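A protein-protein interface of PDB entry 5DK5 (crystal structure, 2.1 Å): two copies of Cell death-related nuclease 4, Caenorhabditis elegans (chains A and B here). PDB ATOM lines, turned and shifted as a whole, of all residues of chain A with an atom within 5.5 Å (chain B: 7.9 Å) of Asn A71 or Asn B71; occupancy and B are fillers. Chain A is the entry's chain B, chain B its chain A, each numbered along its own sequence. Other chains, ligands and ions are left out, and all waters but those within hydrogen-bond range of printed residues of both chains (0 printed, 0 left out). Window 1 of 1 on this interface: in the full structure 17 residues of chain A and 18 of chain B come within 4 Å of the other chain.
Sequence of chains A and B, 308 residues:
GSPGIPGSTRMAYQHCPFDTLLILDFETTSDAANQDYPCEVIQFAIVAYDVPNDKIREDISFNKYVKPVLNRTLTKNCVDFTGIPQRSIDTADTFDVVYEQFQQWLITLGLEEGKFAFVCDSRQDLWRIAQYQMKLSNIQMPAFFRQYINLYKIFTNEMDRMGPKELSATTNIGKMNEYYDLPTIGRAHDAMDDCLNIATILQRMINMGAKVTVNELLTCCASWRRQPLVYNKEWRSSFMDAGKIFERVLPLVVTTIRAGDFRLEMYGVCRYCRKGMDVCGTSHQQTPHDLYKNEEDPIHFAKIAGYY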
ATOM      1  N   THR A  29       1.120 -35.470  -8.905  1.00  0.00           N
ATOM      2  CA  THR A  29       1.558 -35.292 -10.278  1.00  0.00           C
ATOM      3  C   THR A  29       2.981 -35.814 -10.375  1.00  0.00           C
ATOM      4  O   THR A  29       3.701 -35.852  -9.376  1.00  0.00           O
ATOM      5  CB  THR A  29       1.508 -33.822 -10.714  1.00  0.00           C
ATOM      6  OG1 THR A  29       2.271 -33.028  -9.796  1.00  0.00           O
ATOM      7  CG2 THR A  29       0.073 -33.320 -10.744  1.00  0.00           C
ATOM      8  N   TYR A  37      10.895 -32.414 -10.252  1.00  0.00           N
ATOM      9  CA  TYR A  37       9.491 -32.194 -10.560  1.00  0.00           C
ATOM     10  C   TYR A  37       8.748 -31.687  -9.324  1.00  0.00           C
ATOM     11  O   TYR A  37       8.889 -32.259  -8.245  1.00  0.00           O
ATOM     12  CB  TYR A  37       8.864 -33.496 -11.058  1.00  0.00           C
ATOM     13  CG  TYR A  37       7.540 -33.324 -11.764  1.00  0.00           C
ATOM     14  CD1 TYR A  37       6.344 -33.347 -11.057  1.00  0.00           C
ATOM     15  CD2 TYR A  37       7.486 -33.152 -13.140  1.00  0.00           C
ATOM     16  CE1 TYR A  37       5.130 -33.194 -11.704  1.00  0.00           C
ATOM     17  CE2 TYR A  37       6.281 -32.998 -13.792  1.00  0.00           C
ATOM     18  CZ  TYR A  37       5.107 -33.021 -13.072  1.00  0.00           C
ATOM     19  OH  TYR A  37       3.905 -32.868 -13.725  1.00  0.00           O
ATOM     20  N   PRO A  38       7.950 -30.613  -9.474  1.00  0.00           N
ATOM     21  CA  PRO A  38       7.216 -30.048  -8.336  1.00  0.00           C
ATOM     22  C   PRO A  38       5.933 -30.818  -8.039  1.00  0.00           C
ATOM     23  O   PRO A  38       4.837 -30.344  -8.341  1.00  0.00           O
ATOM     24  CB  PRO A  38       6.921 -28.622  -8.801  1.00  0.00           C
ATOM     25  CG  PRO A  38       6.734 -28.763 -10.267  1.00  0.00           C
ATOM     26  CD  PRO A  38       7.702 -29.844 -10.706  1.00  0.00           C
ATOM     27  N   GLU A  40       2.647 -32.203  -6.951  1.00  0.00           N
ATOM     28  CA  GLU A  40       1.450 -31.695  -6.287  1.00  0.00           C
ATOM     29  C   GLU A  40       0.483 -32.834  -5.998  1.00  0.00           C
ATOM     30  O   GLU A  40       0.275 -33.700  -6.843  1.00  0.00           O
ATOM     31  CB  GLU A  40       0.751 -30.647  -7.150  1.00  0.00           C
ATOM     32  CG  GLU A  40       1.574 -29.416  -7.442  1.00  0.00           C
ATOM     33  CD  GLU A  40       0.895 -28.509  -8.445  1.00  0.00           C
ATOM     34  OE1 GLU A  40       0.973 -28.800  -9.657  1.00  0.00           O
ATOM     35  OE2 GLU A  40       0.272 -27.513  -8.020  1.00  0.00           O
ATOM     36  N   PRO A  68      -4.286 -29.791  -9.113  1.00  0.00           N
ATOM     37  CA  PRO A  68      -2.973 -29.134  -9.075  1.00  0.00           C
ATOM     38  C   PRO A  68      -2.989 -27.806  -9.829  1.00  0.00           C
ATOM     39  O   PRO A  68      -3.876 -27.607 -10.656  1.00  0.00           O
ATOM     40  CB  PRO A  68      -2.058 -30.148  -9.760  1.00  0.00           C
ATOM     41  CG  PRO A  68      -2.947 -30.850 -10.717  1.00  0.00           C
ATOM     42  CD  PRO A  68      -4.310 -30.901 -10.085  1.00  0.00           C
ATOM     43  N   VAL A  69      -2.030 -26.922  -9.554  1.00  0.00           N
ATOM     44  CA  VAL A  69      -2.016 -25.587 -10.158  1.00  0.00           C
ATOM     45  C   VAL A  69      -0.720 -25.275 -10.909  1.00  0.00           C
ATOM     46  O   VAL A  69      -0.688 -24.366 -11.737  1.00  0.00           O
ATOM     47  CB  VAL A  69      -2.236 -24.491  -9.093  1.00  0.00           C
ATOM     48  CG1 VAL A  69      -3.601 -24.655  -8.437  1.00  0.00           C
ATOM     49  CG2 VAL A  69      -1.129 -24.522  -8.045  1.00  0.00           C
ATOM     50  N   LEU A  70       0.347 -26.014 -10.615  1.00  0.00           N
ATOM     51  CA  LEU A  70       1.622 -25.822 -11.307  1.00  0.00           C
ATOM     52  C   LEU A  70       1.651 -26.607 -12.616  1.00  0.00           C
ATOM     53  O   LEU A  70       2.081 -26.095 -13.649  1.00  0.00           O
ATOM     54  CB  LEU A  70       2.796 -26.246 -10.422  1.00  0.00           C
ATOM     55  CG  LEU A  70       2.950 -25.520  -9.085  1.00  0.00           C
ATOM     56  CD1 LEU A  70       4.138 -26.083  -8.326  1.00  0.00           C
ATOM     57  CD2 LEU A  70       3.112 -24.024  -9.295  1.00  0.00           C
ATOM     58  N   ASN A  71       1.203 -27.857 -12.551  1.00  0.00           N
ATOM     59  CA  ASN A  71       1.064 -28.708 -13.728  1.00  0.00           C
ATOM     60  C   ASN A  71      -0.340 -29.288 -13.754  1.00  0.00           C
ATOM     61  O   ASN A  71      -0.641 -30.255 -13.055  1.00  0.00           O
ATOM     62  CB  ASN A  71       2.112 -29.817 -13.728  1.00  0.00           C
ATOM     63  CG  ASN A  71       3.520 -29.282 -13.902  1.00  0.00           C
ATOM     64  OD1 ASN A  71       3.919 -28.895 -15.001  1.00  0.00           O
ATOM     65  ND2 ASN A  71       4.282 -29.255 -12.814  1.00  0.00           N
ATOM     66  N   ARG A  72      -1.194 -28.677 -14.566  1.00  0.00           N
ATOM     67  CA  ARG A  72      -2.626 -28.935 -14.517  1.00  0.00           C
ATOM     68  C   ARG A  72      -3.058 -30.079 -15.426  1.00  0.00           C
ATOM     69  O   ARG A  72      -4.174 -30.581 -15.305  1.00  0.00           O
ATOM     70  CB  ARG A  72      -3.383 -27.659 -14.877  1.00  0.00           C
ATOM     71  CG  ARG A  72      -3.033 -26.500 -13.958  1.00  0.00           C
ATOM     72  CD  ARG A  72      -3.708 -25.207 -14.352  1.00  0.00           C
ATOM     73  NE  ARG A  72      -2.975 -24.071 -13.808  1.00  0.00           N
ATOM     74  CZ  ARG A  72      -3.361 -22.804 -13.902  1.00  0.00           C
ATOM     75  NH1 ARG A  72      -4.492 -22.488 -14.520  1.00  0.00           N
ATOM     76  NH2 ARG A  72      -2.613 -21.850 -13.373  1.00  0.00           N
ATOM     77  N   THR A  73      -2.170 -30.486 -16.328  1.00  0.00           N
ATOM     78  CA  THR A  73      -2.413 -31.646 -17.182  1.00  0.00           C
ATOM     79  C   THR A  73      -1.561 -32.815 -16.714  1.00  0.00           C
ATOM     80  O   THR A  73      -0.332 -32.749 -16.758  1.00  0.00           O
ATOM     81  CB  THR A  73      -2.086 -31.359 -18.663  1.00  0.00           C
ATOM     82  OG1 THR A  73      -2.663 -30.111 -19.063  1.00  0.00           O
ATOM     83  CG2 THR A  73      -2.618 -32.475 -19.549  1.00  0.00           C
ATOM     84  N   LEU A  74      -2.209 -33.884 -16.262  1.00  0.00           N
ATOM     85  CA  LEU A  74      -1.489 -35.086 -15.860  1.00  0.00           C
ATOM     86  C   LEU A  74      -0.768 -35.698 -17.055  1.00  0.00           C
ATOM     87  O   LEU A  74      -1.350 -35.854 -18.126  1.00  0.00           O
ATOM     88  CB  LEU A  74      -2.441 -36.116 -15.248  1.00  0.00           C
ATOM     89  CG  LEU A  74      -3.242 -35.701 -14.011  1.00  0.00           C
ATOM     90  CD1 LEU A  74      -4.003 -36.904 -13.474  1.00  0.00           C
ATOM     91  CD2 LEU A  74      -2.342 -35.109 -12.935  1.00  0.00           C
ATOM     92  N   THR B  29       4.863 -26.754 -25.015  1.00  0.00           N
ATOM     93  CA  THR B  29       4.728 -27.807 -24.021  1.00  0.00           C
ATOM     94  C   THR B  29       4.046 -28.990 -24.693  1.00  0.00           C
ATOM     95  O   THR B  29       3.235 -28.803 -25.599  1.00  0.00           O
ATOM     96  CB  THR B  29       3.899 -27.347 -22.812  1.00  0.00           C
ATOM     97  OG1 THR B  29       2.600 -26.931 -23.256  1.00  0.00           O
ATOM     98  CG2 THR B  29       4.584 -26.186 -22.095  1.00  0.00           C
ATOM     99  N   SER B  30       4.369 -30.204 -24.264  1.00  0.00           N
ATOM    100  CA  SER B  30       3.733 -31.381 -24.837  1.00  0.00           C
ATOM    101  C   SER B  30       3.922 -32.633 -23.993  1.00  0.00           C
ATOM    102  O   SER B  30       4.777 -32.689 -23.108  1.00  0.00           O
ATOM    103  CB  SER B  30       4.271 -31.638 -26.248  1.00  0.00           C
ATOM    104  OG  SER B  30       5.672 -31.849 -26.227  1.00  0.00           O
ATOM    105  N   ASP B  36      -4.714 -34.770 -26.025  1.00  0.00           N
ATOM    106  CA  ASP B  36      -5.617 -33.896 -25.285  1.00  0.00           C
ATOM    107  C   ASP B  36      -4.791 -33.082 -24.298  1.00  0.00           C
ATOM    108  O   ASP B  36      -4.890 -33.263 -23.084  1.00  0.00           O
ATOM    109  CB  ASP B  36      -6.701 -34.703 -24.565  1.00  0.00           C
ATOM    110  CG  ASP B  36      -7.812 -33.830 -24.015  1.00  0.00           C
ATOM    111  OD1 ASP B  36      -7.821 -32.615 -24.305  1.00  0.00           O
ATOM    112  OD2 ASP B  36      -8.687 -34.362 -23.298  1.00  0.00           O
ATOM    113  N   TYR B  37      -3.974 -32.186 -24.843  1.00  0.00           N
ATOM    114  CA  TYR B  37      -2.983 -31.459 -24.068  1.00  0.00           C
ATOM    115  C   TYR B  37      -3.021 -29.974 -24.429  1.00  0.00           C
ATOM    116  O   TYR B  37      -2.982 -29.623 -25.609  1.00  0.00           O
ATOM    117  CB  TYR B  37      -1.591 -32.037 -24.327  1.00  0.00           C
ATOM    118  CG  TYR B  37      -0.528 -31.538 -23.378  1.00  0.00           C
ATOM    119  CD1 TYR B  37       0.160 -30.357 -23.631  1.00  0.00           C
ATOM    120  CD2 TYR B  37      -0.209 -32.249 -22.229  1.00  0.00           C
ATOM    121  CE1 TYR B  37       1.132 -29.899 -22.764  1.00  0.00           C
ATOM    122  CE2 TYR B  37       0.760 -31.798 -21.358  1.00  0.00           C
ATOM    123  CZ  TYR B  37       1.428 -30.623 -21.629  1.00  0.00           C
ATOM    124  OH  TYR B  37       2.394 -30.173 -20.762  1.00  0.00           O
ATOM    125  N   PRO B  38      -3.103 -29.094 -23.415  1.00  0.00           N
ATOM    126  CA  PRO B  38      -3.202 -27.660 -23.696  1.00  0.00           C
ATOM    127  C   PRO B  38      -1.844 -27.049 -24.046  1.00  0.00           C
ATOM    128  O   PRO B  38      -1.253 -26.346 -23.225  1.00  0.00           O
ATOM    129  CB  PRO B  38      -3.753 -27.098 -22.386  1.00  0.00           C
ATOM    130  CG  PRO B  38      -3.152 -27.983 -21.342  1.00  0.00           C
ATOM    131  CD  PRO B  38      -3.079 -29.362 -21.964  1.00  0.00           C
ATOM    132  N   CYS B  39      -1.364 -27.332 -25.256  1.00  0.00           N
ATOM    133  CA  CYS B  39      -0.066 -26.852 -25.731  1.00  0.00           C
ATOM    134  C   CYS B  39       0.125 -25.344 -25.560  1.00  0.00           C
ATOM    135  O   CYS B  39      -0.696 -24.552 -26.018  1.00  0.00           O
ATOM    136  CB  CYS B  39       0.119 -27.220 -27.208  1.00  0.00           C
ATOM    137  SG  CYS B  39       0.062 -28.993 -27.542  1.00  0.00           S
ATOM    138  N   GLU B  40       1.219 -24.970 -24.899  1.00  0.00           N
ATOM    139  CA  GLU B  40       1.608 -23.571 -24.708  1.00  0.00           C
ATOM    140  C   GLU B  40       2.942 -23.293 -25.384  1.00  0.00           C
ATOM    141  O   GLU B  40       3.865 -24.093 -25.278  1.00  0.00           O
ATOM    142  CB  GLU B  40       1.725 -23.231 -23.220  1.00  0.00           C
ATOM    143  CG  GLU B  40       0.411 -23.190 -22.472  1.00  0.00           C
ATOM    144  CD  GLU B  40       0.598 -22.865 -21.003  1.00  0.00           C
ATOM    145  OE1 GLU B  40       0.942 -23.785 -20.230  1.00  0.00           O
ATOM    146  OE2 GLU B  40       0.414 -21.688 -20.621  1.00  0.00           O
ATOM    147  N   ILE B  42       6.574 -22.234 -25.931  1.00  0.00           N
ATOM    148  CA  ILE B  42       7.731 -22.129 -25.042  1.00  0.00           C
ATOM    149  C   ILE B  42       8.974 -21.622 -25.776  1.00  0.00           C
ATOM    150  O   ILE B  42       9.970 -21.277 -25.142  1.00  0.00           O
ATOM    151  CB  ILE B  42       8.046 -23.478 -24.365  1.00  0.00           C
ATOM    152  CG1 ILE B  42       8.207 -24.585 -25.410  1.00  0.00           C
ATOM    153  CG2 ILE B  42       6.936 -23.833 -23.379  1.00  0.00           C
ATOM    154  CD1 ILE B  42       8.629 -25.922 -24.822  1.00  0.00           C
ATOM    155  N   LYS B  67       7.504 -18.438 -21.095  1.00  0.00           N
ATOM    156  CA  LYS B  67       7.125 -19.146 -19.874  1.00  0.00           C
ATOM    157  C   LYS B  67       5.662 -19.590 -19.929  1.00  0.00           C
ATOM    158  O   LYS B  67       4.767 -18.748 -19.981  1.00  0.00           O
ATOM    159  CB  LYS B  67       7.341 -18.263 -18.641  1.00  0.00           C
ATOM    160  CG  LYS B  67       7.034 -18.974 -17.321  1.00  0.00           C
ATOM    161  CD  LYS B  67       6.617 -18.005 -16.227  1.00  0.00           C
ATOM    162  CE  LYS B  67       7.758 -17.116 -15.778  1.00  0.00           C
ATOM    163  NZ  LYS B  67       8.945 -17.891 -15.322  1.00  0.00           N
ATOM    164  N   PRO B  68       5.409 -20.912 -19.904  1.00  0.00           N
ATOM    165  CA  PRO B  68       4.024 -21.401 -19.853  1.00  0.00           C
ATOM    166  C   PRO B  68       3.434 -21.284 -18.446  1.00  0.00           C
ATOM    167  O   PRO B  68       4.200 -21.164 -17.492  1.00  0.00           O
ATOM    168  CB  PRO B  68       4.158 -22.862 -20.278  1.00  0.00           C
ATOM    169  CG  PRO B  68       5.507 -23.255 -19.790  1.00  0.00           C
ATOM    170  CD  PRO B  68       6.378 -22.023 -19.899  1.00  0.00           C
ATOM    171  N   VAL B  69       2.107 -21.328 -18.320  1.00  0.00           N
ATOM    172  CA  VAL B  69       1.454 -21.146 -17.021  1.00  0.00           C
ATOM    173  C   VAL B  69       0.514 -22.291 -16.631  1.00  0.00           C
ATOM    174  O   VAL B  69       0.209 -22.464 -15.452  1.00  0.00           O
ATOM    175  CB  VAL B  69       0.651 -19.828 -16.985  1.00  0.00           C
ATOM    176  CG1 VAL B  69       1.584 -18.644 -17.169  1.00  0.00           C
ATOM    177  CG2 VAL B  69      -0.437 -19.817 -18.051  1.00  0.00           C
ATOM    178  N   LEU B  70       0.051 -23.063 -17.611  1.00  0.00           N
ATOM    179  CA  LEU B  70      -0.834 -24.194 -17.332  1.00  0.00           C
ATOM    180  C   LEU B  70      -0.024 -25.414 -16.909  1.00  0.00           C
ATOM    181  O   LEU B  70      -0.393 -26.127 -15.972  1.00  0.00           O
ATOM    182  CB  LEU B  70      -1.692 -24.534 -18.551  1.00  0.00           C
ATOM    183  CG  LEU B  70      -2.569 -23.410 -19.107  1.00  0.00           C
ATOM    184  CD1 LEU B  70      -3.364 -23.904 -20.304  1.00  0.00           C
ATOM    185  CD2 LEU B  70      -3.503 -22.864 -18.044  1.00  0.00           C
ATOM    186  N   ASN B  71       1.075 -25.651 -17.616  1.00  0.00           N
ATOM    187  CA  ASN B  71       2.015 -26.710 -17.272  1.00  0.00           C
ATOM    188  C   ASN B  71       3.424 -26.148 -17.258  1.00  0.00           C
ATOM    189  O   ASN B  71       4.072 -26.028 -18.300  1.00  0.00           O
ATOM    190  CB  ASN B  71       1.906 -27.874 -18.253  1.00  0.00           C
ATOM    191  CG  ASN B  71       0.557 -28.562 -18.184  1.00  0.00           C
ATOM    192  OD1 ASN B  71       0.276 -29.309 -17.246  1.00  0.00           O
ATOM    193  ND2 ASN B  71      -0.287 -28.312 -19.177  1.00  0.00           N
ATOM    194  N   ARG B  72       3.887 -25.808 -16.060  1.00  0.00           N
ATOM    195  CA  ARG B  72       5.103 -25.028 -15.887  1.00  0.00           C
ATOM    196  C   ARG B  72       6.362 -25.890 -15.892  1.00  0.00           C
ATOM    197  O   ARG B  72       7.474 -25.370 -16.010  1.00  0.00           O
ATOM    198  CB  ARG B  72       5.013 -24.227 -14.588  1.00  0.00           C
ATOM    199  CG  ARG B  72       3.847 -23.243 -14.567  1.00  0.00           C
ATOM    200  CD  ARG B  72       3.735 -22.513 -13.240  1.00  0.00           C
ATOM    201  NE  ARG B  72       4.935 -21.740 -12.933  1.00  0.00           N
ATOM    202  CZ  ARG B  72       5.093 -21.005 -11.836  1.00  0.00           C
ATOM    203  NH1 ARG B  72       4.125 -20.936 -10.931  1.00  0.00           N
ATOM    204  NH2 ARG B  72       6.220 -20.338 -11.642  1.00  0.00           N
ATOM    205  N   THR B  73       6.185 -27.202 -15.766  1.00  0.00           N
ATOM    206  CA  THR B  73       7.303 -28.141 -15.803  1.00  0.00           C
ATOM    207  C   THR B  73       7.259 -28.949 -17.090  1.00  0.00           C
ATOM    208  O   THR B  73       6.303 -29.681 -17.346  1.00  0.00           O
ATOM    209  CB  THR B  73       7.277 -29.093 -14.599  1.00  0.00           C
ATOM    210  OG1 THR B  73       7.189 -28.327 -13.394  1.00  0.00           O
ATOM    211  CG2 THR B  73       8.536 -29.950 -14.551  1.00  0.00           C
ATOM    212  N   LEU B  74       8.299 -28.803 -17.905  1.00  0.00           N
ATOM    213  CA  LEU B  74       8.381 -29.531 -19.160  1.00  0.00           C
ATOM    214  C   LEU B  74       8.522 -31.022 -18.900  1.00  0.00           C
ATOM    215  O   LEU B  74       9.335 -31.441 -18.080  1.00  0.00           O
ATOM    216  CB  LEU B  74       9.562 -29.036 -19.998  1.00  0.00           C
ATOM    217  CG  LEU B  74       9.582 -27.552 -20.371  1.00  0.00           C
ATOM    218  CD1 LEU B  74      10.774 -27.259 -21.272  1.00  0.00           C
ATOM    219  CD2 LEU B  74       8.290 -27.140 -21.051  1.00  0.00           C
ATOM    220  N   THR B  75       7.715 -31.820 -19.589  1.00  0.00           N
ATOM    221  CA  THR B  75       7.881 -33.266 -19.561  1.00  0.00           C
ATOM    222  C   THR B  75       9.218 -33.609 -20.188  1.00  0.00           C
ATOM    223  O   THR B  75       9.730 -32.851 -21.013  1.00  0.00           O
ATOM    224  CB  THR B  75       6.767 -33.998 -20.319  1.00  0.00           C
ATOM    225  OG1 THR B  75       6.857 -33.685 -21.718  1.00  0.00           O
ATOM    226  CG2 THR B  75       5.394 -33.602 -19.785  1.00  0.00           C
ATOM    227  N   GLN B  86      14.626 -26.732 -18.867  1.00  0.00           N
ATOM    228  CA  GLN B  86      13.648 -26.172 -17.941  1.00  0.00           C
ATOM    229  C   GLN B  86      14.064 -24.786 -17.459  1.00  0.00           C
ATOM    230  O   GLN B  86      13.224 -23.906 -17.276  1.00  0.00           O
ATOM    231  CB  GLN B  86      13.458 -27.108 -16.745  1.00  0.00           C
ATOM    232  CG  GLN B  86      12.417 -26.648 -15.731  1.00  0.00           C
ATOM    233  CD  GLN B  86      11.017 -26.587 -16.308  1.00  0.00           C
ATOM    234  OE1 GLN B  86      10.584 -27.494 -17.021  1.00  0.00           O
ATOM    235  NE2 GLN B  86      10.296 -25.515 -15.999  1.00  0.00           N
ATOM    236  N   ILE B  89      12.949 -21.703 -19.624  1.00  0.00           N
ATOM    237  CA  ILE B  89      11.562 -21.239 -19.569  1.00  0.00           C
ATOM    238  C   ILE B  89      11.235 -20.659 -18.191  1.00  0.00           C
ATOM    239  O   ILE B  89      10.320 -19.846 -18.056  1.00  0.00           O
ATOM    240  CB  ILE B  89      10.546 -22.370 -19.918  1.00  0.00           C
ATOM    241  CG1 ILE B  89      10.381 -23.385 -18.776  1.00  0.00           C
ATOM    242  CG2 ILE B  89      10.961 -23.077 -21.202  1.00  0.00           C
ATOM    243  CD1 ILE B  89       9.188 -24.305 -18.967  1.00  0.00           C
ATOM    244  N   HIS B 300     -10.283 -32.073 -22.426  1.00  0.00           N
ATOM    245  CA  HIS B 300      -9.521 -31.292 -21.456  1.00  0.00           C
ATOM    246  C   HIS B 300      -8.970 -29.986 -22.027  1.00  0.00           C
ATOM    247  O   HIS B 300      -9.101 -28.935 -21.398  1.00  0.00           O
ATOM    248  CB  HIS B 300      -8.365 -32.128 -20.900  1.00  0.00           C
ATOM    249  CG  HIS B 300      -7.411 -31.350 -20.050  1.00  0.00           C
ATOM    250  ND1 HIS B 300      -7.774 -30.776 -18.849  1.00  0.00           N
ATOM    251  CD2 HIS B 300      -6.100 -31.049 -20.228  1.00  0.00           C
ATOM    252  CE1 HIS B 300      -6.731 -30.156 -18.328  1.00  0.00           C
ATOM    253  NE2 HIS B 300      -5.706 -30.306 -19.141  1.00  0.00           N
ATOM    254  N   ILE B 304     -10.114 -26.297 -20.419  1.00  0.00           N
ATOM    255  CA  ILE B 304      -9.177 -25.463 -19.674  1.00  0.00           C
ATOM    256  C   ILE B 304      -8.900 -24.153 -20.412  1.00  0.00           C
ATOM    257  O   ILE B 304      -8.490 -23.162 -19.805  1.00  0.00           O
ATOM    258  CB  ILE B 304      -7.849 -26.211 -19.417  1.00  0.00           C
ATOM    259  CG1 ILE B 304      -7.027 -25.498 -18.337  1.00  0.00           C
ATOM    260  CG2 ILE B 304      -7.057 -26.362 -20.715  1.00  0.00           C
ATOM    261  CD1 ILE B 304      -5.851 -26.318 -17.820  1.00  0.00           C
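OD2 of Asp B36 lies within hydrogen-bond range of N of His B300, at 2.9 Å. The side-chain sulfur of Cys B39 lies within hydrogen-bond range of the backbone carbonyl oxygen of Tyr B37, at 3.7 Å. The backbone NH (N) of Asn B71 is in hydrogen-bond range of the side-chain carboxylate (OE1) of Glu B40 (3.2 Å). NE2 of Gln B86 lies within hydrogen-bond range of O of Arg B72. N of Leu A70 lies within hydrogen-bond range of OE2 of Glu A40, 3.0 Å away. The guanidinium group (NE) of Arg A72 sits at hydrogen-bond distance from the backbone carbonyl oxygen (O) of Val A69, at 3.1 Å.
Of the printed residues of chain B, Asn A71 touches Leu B70, Asn B71, Arg B72 and Thr B73. Of the printed residues of chain A, Asn B71 touches Leu A70 (3.7 Å), Asn A71 (3.5 Å), Arg A72 (3.1 Å) and Thr A73 (2.9 Å). Printed residues of chain B within 4 Å of Pro A38: Thr B73. Of the printed residues of chain B, Leu A70 touches Leu B70, Asn B71 and Arg B72. Of the printed residues of chain A, Thr B73 touches Tyr A37 (3.7 Å), Pro A38 (3.1 Å) and Asn A71 (2.9 Å). The nearest residue of chain B that does not touch Asn A71 is Leu B74 (5.3 Å). The nearest residue of chain A that does not touch Asn B71 is Leu A74 (5.3 Å).
Leu B70 touches its own counterpart, Leu A70. Leu A70 touches Asn B71, and with the chains exchanged Asn A71 touches Leu B70. Asn A71 touches Arg B72, and with the chains exchanged Arg A72 touches Asn B71. Arg A72 touches Val B69, but with the chains exchanged Val A69 does not touch Arg B72 (5.0 Å). Positions printed for both chains: 29, 37, 38, 40, 68, 69, 70, 71, 72, 73 and 74. Of the 17 pairs that touch across the chains among the printed residues, 14 have their exchanged pair printed and touching as well.
CD2 of Tyr A37 touches CG2 of Thr B73, 3.7 Å away. Thr B73 touches Pro A38 (OG1 to CD, 3.1 Å). Leu A70 touches Asn B71 (O to CA, 3.7 Å). Asn A71 touches Leu B70 (CA to O, 3.7 Å). C of Asn A71 touches OD1 of Asn B71 (3.5 Å). Val B69 touches Arg A72. His B300 touches Arg A72 (CE1 to O, 3.98 Å). Tyr B37 touches Thr A73. CD of Pro B38 touches OG1 of Thr A73, at 3.0 Å.
N of Arg A72 lies within hydrogen-bond range of O of Leu B70 (3.0 Å). The backbone NH (N) of Arg A72 sits at hydrogen-bond distance from the side-chain amide oxygen (OD1) of Asn B71. OD1 of Asn B71 lies within hydrogen-bond range of N of Thr A73 (2.9 Å). The backbone NH (N) of Arg B72 is in hydrogen-bond range of the backbone carbonyl oxygen (O) of Leu A70, at 3.0 Å. The side-chain amide oxygen (OD1) of Asn A71 lies within hydrogen-bond range of the backbone NH (N) of Arg B72 (3.3 Å). The side-chain amide oxygen (OD1) of Asn A71 sits at hydrogen-bond distance from the backbone NH (N) of Thr B73 (2.9 Å). The side-chain hydroxyl (OG1) of Thr A73 lies within hydrogen-bond range of a ring nitrogen (NE2) of His B300 (3.1 Å). The backbone carbonyl oxygen (O) of Leu A70 lies close to the backbone carbonyl oxygen (O) of Leu B70, 3.4 Å away.
Of the 21 printed residues of chain B, 8 touch a printed residue of chain A. Hydrophobic or aromatic side chains of chain B that line the printed part of chain A: Tyr B37, Pro B38, Leu B70 and His B300. Hydrophobic or aromatic side chains of chain A within 4 Å of the printed part of chain B: Tyr A37, Pro A38 and Leu A70.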
